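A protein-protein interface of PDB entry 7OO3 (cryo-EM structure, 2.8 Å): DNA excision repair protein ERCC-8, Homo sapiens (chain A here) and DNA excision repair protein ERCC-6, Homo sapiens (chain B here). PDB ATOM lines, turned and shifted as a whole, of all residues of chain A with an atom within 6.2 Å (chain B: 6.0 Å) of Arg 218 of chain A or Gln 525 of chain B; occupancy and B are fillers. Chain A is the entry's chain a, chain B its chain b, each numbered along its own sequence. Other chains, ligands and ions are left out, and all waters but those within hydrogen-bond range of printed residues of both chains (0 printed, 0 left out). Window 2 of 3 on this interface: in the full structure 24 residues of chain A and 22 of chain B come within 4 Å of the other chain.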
ATOM      1  N   HIS A 180      19.942   7.954  -9.816  1.00  0.00           N
ATOM      2  CA  HIS A 180      19.095   8.525 -10.857  1.00  0.00           C
ATOM      3  C   HIS A 180      19.088  10.041 -10.765  1.00  0.00           C
ATOM      4  O   HIS A 180      18.952  10.609  -9.679  1.00  0.00           O
ATOM      5  CB  HIS A 180      17.673   7.993 -10.720  1.00  0.00           C
ATOM      6  CG  HIS A 180      16.815   8.243 -11.920  1.00  0.00           C
ATOM      7  ND1 HIS A 180      16.433   9.506 -12.313  1.00  0.00           N
ATOM      8  CD2 HIS A 180      16.220   7.387 -12.782  1.00  0.00           C
ATOM      9  CE1 HIS A 180      15.672   9.419 -13.387  1.00  0.00           C
ATOM     10  NE2 HIS A 180      15.524   8.144 -13.690  1.00  0.00           N
ATOM     11  N   LEU A 182      17.596  13.617 -12.964  1.00  0.00           N
ATOM     12  CA  LEU A 182      16.821  14.252 -14.021  1.00  0.00           C
ATOM     13  C   LEU A 182      17.537  15.541 -14.391  1.00  0.00           C
ATOM     14  O   LEU A 182      17.567  16.488 -13.599  1.00  0.00           O
ATOM     15  CB  LEU A 182      15.391  14.529 -13.565  1.00  0.00           C
ATOM     16  CG  LEU A 182      14.627  13.390 -12.890  1.00  0.00           C
ATOM     17  CD1 LEU A 182      13.513  13.945 -12.033  1.00  0.00           C
ATOM     18  CD2 LEU A 182      14.064  12.454 -13.936  1.00  0.00           C
ATOM     19  N   ASP A 215       8.383  12.763 -16.005  1.00  0.00           N
ATOM     20  CA  ASP A 215       7.812  11.434 -15.844  1.00  0.00           C
ATOM     21  C   ASP A 215       9.020  10.557 -15.542  1.00  0.00           C
ATOM     22  O   ASP A 215       9.715  10.106 -16.453  1.00  0.00           O
ATOM     23  CB  ASP A 215       7.056  10.995 -17.097  1.00  0.00           C
ATOM     24  CG  ASP A 215       6.426   9.623 -16.958  1.00  0.00           C
ATOM     25  OD1 ASP A 215       6.741   8.900 -15.992  1.00  0.00           O
ATOM     26  OD2 ASP A 215       5.605   9.265 -17.827  1.00  0.00           O
ATOM     27  N   VAL A 216       9.275  10.337 -14.250  1.00  0.00           N
ATOM     28  CA  VAL A 216      10.522   9.719 -13.814  1.00  0.00           C
ATOM     29  C   VAL A 216      10.721   8.335 -14.416  1.00  0.00           C
ATOM     30  O   VAL A 216      11.853   7.844 -14.466  1.00  0.00           O
ATOM     31  CB  VAL A 216      10.575   9.674 -12.272  1.00  0.00           C
ATOM     32  CG1 VAL A 216      10.489  11.077 -11.700  1.00  0.00           C
ATOM     33  CG2 VAL A 216       9.461   8.804 -11.705  1.00  0.00           C
ATOM     34  N   ARG A 217       9.649   7.685 -14.871  1.00  0.00           N
ATOM     35  CA  ARG A 217       9.809   6.472 -15.665  1.00  0.00           C
ATOM     36  C   ARG A 217      10.481   6.776 -16.992  1.00  0.00           C
ATOM     37  O   ARG A 217      11.335   6.013 -17.456  1.00  0.00           O
ATOM     38  CB  ARG A 217       8.452   5.831 -15.929  1.00  0.00           C
ATOM     39  CG  ARG A 217       7.673   5.443 -14.703  1.00  0.00           C
ATOM     40  CD  ARG A 217       6.357   4.770 -15.073  1.00  0.00           C
ATOM     41  NE  ARG A 217       5.538   5.583 -15.974  1.00  0.00           N
ATOM     42  CZ  ARG A 217       4.213   5.515 -16.072  1.00  0.00           C
ATOM     43  NH1 ARG A 217       3.508   4.663 -15.336  1.00  0.00           N
ATOM     44  NH2 ARG A 217       3.583   6.307 -16.926  1.00  0.00           N
ATOM     45  N   ARG A 218      10.101   7.885 -17.614  1.00  0.00           N
ATOM     46  CA  ARG A 218      10.568   8.213 -18.947  1.00  0.00           C
ATOM     47  C   ARG A 218      12.072   8.451 -18.939  1.00  0.00           C
ATOM     48  O   ARG A 218      12.648   8.909 -17.950  1.00  0.00           O
ATOM     49  CB  ARG A 218       9.832   9.448 -19.458  1.00  0.00           C
ATOM     50  CG  ARG A 218       9.966   9.689 -20.955  1.00  0.00           C
ATOM     51  CD  ARG A 218       8.775  10.442 -21.571  1.00  0.00           C
ATOM     52  NE  ARG A 218       7.471   9.910 -21.174  1.00  0.00           N
ATOM     53  CZ  ARG A 218       6.302  10.361 -21.620  1.00  0.00           C
ATOM     54  NH1 ARG A 218       6.245  11.355 -22.497  1.00  0.00           N
ATOM     55  NH2 ARG A 218       5.177   9.806 -21.190  1.00  0.00           N
ATOM     56  N   ALA A 219      12.709   8.125 -20.061  1.00  0.00           N
ATOM     57  CA  ALA A 219      14.149   8.267 -20.229  1.00  0.00           C
ATOM     58  C   ALA A 219      14.502   9.348 -21.245  1.00  0.00           C
ATOM     59  O   ALA A 219      15.566   9.292 -21.865  1.00  0.00           O
ATOM     60  CB  ALA A 219      14.762   6.933 -20.648  1.00  0.00           C
ATOM     61  N   SER A 220      13.626  10.344 -21.416  1.00  0.00           N
ATOM     62  CA  SER A 220      13.787  11.329 -22.479  1.00  0.00           C
ATOM     63  C   SER A 220      13.481  12.743 -21.998  1.00  0.00           C
ATOM     64  O   SER A 220      12.952  13.558 -22.762  1.00  0.00           O
ATOM     65  CB  SER A 220      12.894  10.994 -23.672  1.00  0.00           C
ATOM     66  OG  SER A 220      11.525  11.095 -23.326  1.00  0.00           O
ATOM     67  N   GLY A 221      13.805  13.055 -20.749  1.00  0.00           N
ATOM     68  CA  GLY A 221      13.726  14.423 -20.287  1.00  0.00           C
ATOM     69  C   GLY A 221      12.339  14.831 -19.829  1.00  0.00           C
ATOM     70  O   GLY A 221      11.412  14.027 -19.702  1.00  0.00           O
ATOM     71  N   LEU A 223       8.645  16.250 -19.366  1.00  0.00           N
ATOM     72  CA  LEU A 223       7.426  16.234 -20.162  1.00  0.00           C
ATOM     73  C   LEU A 223       7.118  17.621 -20.704  1.00  0.00           C
ATOM     74  O   LEU A 223       6.925  17.805 -21.911  1.00  0.00           O
ATOM     75  CB  LEU A 223       6.253  15.746 -19.312  1.00  0.00           C
ATOM     76  CG  LEU A 223       6.117  14.273 -18.935  1.00  0.00           C
ATOM     77  CD1 LEU A 223       4.803  14.078 -18.206  1.00  0.00           C
ATOM     78  CD2 LEU A 223       6.193  13.358 -20.134  1.00  0.00           C
ATOM     79  N   GLU B 520       7.011  -3.747 -21.601  1.00  0.00           N
ATOM     80  CA  GLU B 520       6.984  -2.979 -20.362  1.00  0.00           C
ATOM     81  C   GLU B 520       7.900  -1.770 -20.467  1.00  0.00           C
ATOM     82  O   GLU B 520       7.533  -0.661 -20.056  1.00  0.00           O
ATOM     83  CB  GLU B 520       7.381  -3.859 -19.177  1.00  0.00           C
ATOM     84  CG  GLU B 520       6.380  -4.957 -18.857  1.00  0.00           C
ATOM     85  CD  GLU B 520       6.814  -5.824 -17.694  1.00  0.00           C
ATOM     86  OE1 GLU B 520       7.952  -5.647 -17.213  1.00  0.00           O
ATOM     87  OE2 GLU B 520       6.021  -6.690 -17.272  1.00  0.00           O
ATOM     88  N   LEU B 521       9.093  -1.961 -21.033  1.00  0.00           N
ATOM     89  CA  LEU B 521       9.975  -0.823 -21.271  1.00  0.00           C
ATOM     90  C   LEU B 521       9.315   0.197 -22.189  1.00  0.00           C
ATOM     91  O   LEU B 521       9.401   1.406 -21.951  1.00  0.00           O
ATOM     92  CB  LEU B 521      11.298  -1.293 -21.871  1.00  0.00           C
ATOM     93  CG  LEU B 521      12.197  -2.222 -21.058  1.00  0.00           C
ATOM     94  CD1 LEU B 521      13.509  -2.389 -21.787  1.00  0.00           C
ATOM     95  CD2 LEU B 521      12.439  -1.711 -19.642  1.00  0.00           C
ATOM     96  N   HIS B 522       8.650  -0.274 -23.244  1.00  0.00           N
ATOM     97  CA  HIS B 522       8.014   0.647 -24.180  1.00  0.00           C
ATOM     98  C   HIS B 522       6.906   1.450 -23.510  1.00  0.00           C
ATOM     99  O   HIS B 522       6.692   2.617 -23.854  1.00  0.00           O
ATOM    100  CB  HIS B 522       7.453  -0.119 -25.378  1.00  0.00           C
ATOM    101  CG  HIS B 522       6.758   0.752 -26.378  1.00  0.00           C
ATOM    102  ND1 HIS B 522       7.439   1.597 -27.226  1.00  0.00           N
ATOM    103  CD2 HIS B 522       5.444   0.915 -26.658  1.00  0.00           C
ATOM    104  CE1 HIS B 522       6.574   2.240 -27.990  1.00  0.00           C
ATOM    105  NE2 HIS B 522       5.358   1.845 -27.665  1.00  0.00           N
ATOM    106  N   CYS B 523       6.191   0.846 -22.559  1.00  0.00           N
ATOM    107  CA  CYS B 523       5.186   1.597 -21.810  1.00  0.00           C
ATOM    108  C   CYS B 523       5.838   2.613 -20.885  1.00  0.00           C
ATOM    109  O   CYS B 523       5.391   3.762 -20.801  1.00  0.00           O
ATOM    110  CB  CYS B 523       4.302   0.650 -21.008  1.00  0.00           C
ATOM    111  SG  CYS B 523       3.208  -0.343 -22.012  1.00  0.00           S
ATOM    112  N   GLN B 524       6.892   2.207 -20.177  1.00  0.00           N
ATOM    113  CA  GLN B 524       7.645   3.153 -19.365  1.00  0.00           C
ATOM    114  C   GLN B 524       8.477   4.114 -20.204  1.00  0.00           C
ATOM    115  O   GLN B 524       9.048   5.054 -19.644  1.00  0.00           O
ATOM    116  CB  GLN B 524       8.547   2.401 -18.386  1.00  0.00           C
ATOM    117  CG  GLN B 524       7.805   1.424 -17.488  1.00  0.00           C
ATOM    118  CD  GLN B 524       8.737   0.609 -16.618  1.00  0.00           C
ATOM    119  OE1 GLN B 524       9.485  -0.234 -17.111  1.00  0.00           O
ATOM    120  NE2 GLN B 524       8.698   0.857 -15.315  1.00  0.00           N
ATOM    121  N   GLN B 525       8.562   3.900 -21.519  1.00  0.00           N
ATOM    122  CA  GLN B 525       9.337   4.761 -22.415  1.00  0.00           C
ATOM    123  C   GLN B 525      10.805   4.797 -22.006  1.00  0.00           C
ATOM    124  O   GLN B 525      11.450   5.847 -22.028  1.00  0.00           O
ATOM    125  CB  GLN B 525       8.751   6.173 -22.470  1.00  0.00           C
ATOM    126  CG  GLN B 525       7.367   6.237 -23.084  1.00  0.00           C
ATOM    127  CD  GLN B 525       7.193   7.425 -24.004  1.00  0.00           C
ATOM    128  OE1 GLN B 525       7.468   8.561 -23.627  1.00  0.00           O
ATOM    129  NE2 GLN B 525       6.731   7.167 -25.221  1.00  0.00           N
ATOM    130  N   ALA B 526      11.334   3.639 -21.624  1.00  0.00           N
ATOM    131  CA  ALA B 526      12.727   3.471 -21.242  1.00  0.00           C
ATOM    132  C   ALA B 526      13.380   2.415 -22.125  1.00  0.00           C
ATOM    133  O   ALA B 526      12.712   1.676 -22.852  1.00  0.00           O
ATOM    134  CB  ALA B 526      12.845   3.078 -19.766  1.00  0.00           C
ATOM    135  N   GLY B 527      14.713   2.363 -22.062  1.00  0.00           N
ATOM    136  CA  GLY B 527      15.488   1.391 -22.801  1.00  0.00           C
ATOM    137  C   GLY B 527      15.996   0.272 -21.904  1.00  0.00           C
ATOM    138  O   GLY B 527      15.854   0.303 -20.686  1.00  0.00           O
ATOM    139  N   PRO B 668      13.321   7.873 -26.783  1.00  0.00           N
ATOM    140  CA  PRO B 668      13.377   7.160 -25.496  1.00  0.00           C
ATOM    141  C   PRO B 668      13.730   5.693 -25.630  1.00  0.00           C
ATOM    142  O   PRO B 668      14.138   5.080 -24.637  1.00  0.00           O
ATOM    143  CB  PRO B 668      11.959   7.334 -24.934  1.00  0.00           C
ATOM    144  CG  PRO B 668      11.118   7.613 -26.122  1.00  0.00           C
ATOM    145  CD  PRO B 668      11.979   8.432 -27.017  1.00  0.00           C
ATOM    146  N   HIS B 669      13.593   5.116 -26.820  1.00  0.00           N
ATOM    147  CA  HIS B 669      13.644   3.670 -27.015  1.00  0.00           C
ATOM    148  C   HIS B 669      15.046   3.279 -27.465  1.00  0.00           C
ATOM    149  O   HIS B 669      15.427   3.504 -28.616  1.00  0.00           O
ATOM    150  CB  HIS B 669      12.591   3.243 -28.029  1.00  0.00           C
ATOM    151  CG  HIS B 669      11.197   3.633 -27.647  1.00  0.00           C
ATOM    152  ND1 HIS B 669      10.433   4.498 -28.401  1.00  0.00           N
ATOM    153  CD2 HIS B 669      10.432   3.284 -26.586  1.00  0.00           C
ATOM    154  CE1 HIS B 669       9.256   4.660 -27.823  1.00  0.00           C
ATOM    155  NE2 HIS B 669       9.230   3.934 -26.719  1.00  0.00           N
ATOM    156  N   PHE B 693      19.573   4.492 -20.974  1.00  0.00           N
ATOM    157  CA  PHE B 693      18.803   5.316 -20.043  1.00  0.00           C
ATOM    158  C   PHE B 693      19.757   6.408 -19.576  1.00  0.00           C
ATOM    159  O   PHE B 693      20.593   6.168 -18.692  1.00  0.00           O
ATOM    160  CB  PHE B 693      18.281   4.497 -18.865  1.00  0.00           C
ATOM    161  CG  PHE B 693      17.135   5.135 -18.132  1.00  0.00           C
ATOM    162  CD1 PHE B 693      17.269   6.370 -17.529  1.00  0.00           C
ATOM    163  CD2 PHE B 693      15.905   4.507 -18.082  1.00  0.00           C
ATOM    164  CE1 PHE B 693      16.207   6.949 -16.870  1.00  0.00           C
ATOM    165  CE2 PHE B 693      14.845   5.081 -17.421  1.00  0.00           C
ATOM    166  CZ  PHE B 693      14.995   6.302 -16.814  1.00  0.00           C
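The backbone carbonyl oxygen (O) of Gln 525 of chain B sits at hydrogen-bond distance from the backbone NH (N) of Ala 219 of chain A, at 3.3 Å. O of Arg 217 of chain A lies close to O of Gln 524 of chain B, at 3.3 Å. The guanidinium group (NE) of Arg 218 of chain A sits at hydrogen-bond distance from the side-chain amide oxygen (OE1) of Gln 525 of chain B, 2.8 Å away.
OD1 of Asp 215 of chain A lies within salt-bridge range of NE of Arg 217 of chain A (3.5 Å). The side-chain carboxylate of Asp 215 of chain A is in salt-bridge range of the guanidinium group of Arg 218 of chain A (3.4 Å).
Among the printed residues, pairs that only touch across the chains: His 180 of chain A with Phe 693 of chain B, Arg 217 of chain A with Phe 693 of chain B, Arg 218 of chain A with Gln 524 of chain B, Arg 218 of chain A with Phe 693 of chain B, Ala 219 of chain A with Phe 693 of chain B and Ser 220 of chain A with Pro 668 of chain B.
Of chain A, only Arg 218 and Ala 219 come within 4 Å of Gln 525 of chain B. Printed residues of chain A within 4 Å of Phe 693 of chain B: His 180, Arg 217, Arg 218 and Ala 219. Of the printed residues of chain B, His 180 of chain A touches Phe 693 (3.5 Å). The nearest residue of chain B that does not touch Arg 218 of chain A is Pro 668 of chain B (5.0 Å). The nearest residue of chain A that does not touch Gln 525 of chain B is Arg 217 of chain A (4.6 Å).
Of the 11 printed residues of chain B, 4 touch a printed residue of chain A. Printed residues of chain B that touch a printed residue of chain A: Gln 524, Gln 525, Pro 668 and Phe 693. Hydrophobic or aromatic side chains of chain B within 4 Å of the printed part of chain A: Pro 668 and Phe 693. Of the 10 printed residues of chain A, 5 touch a printed residue of chain B. Among the printed residues, no Asp or Glu carboxylate lies within 4 Å of a Lys or Arg side-chain nitrogen of the other chain.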
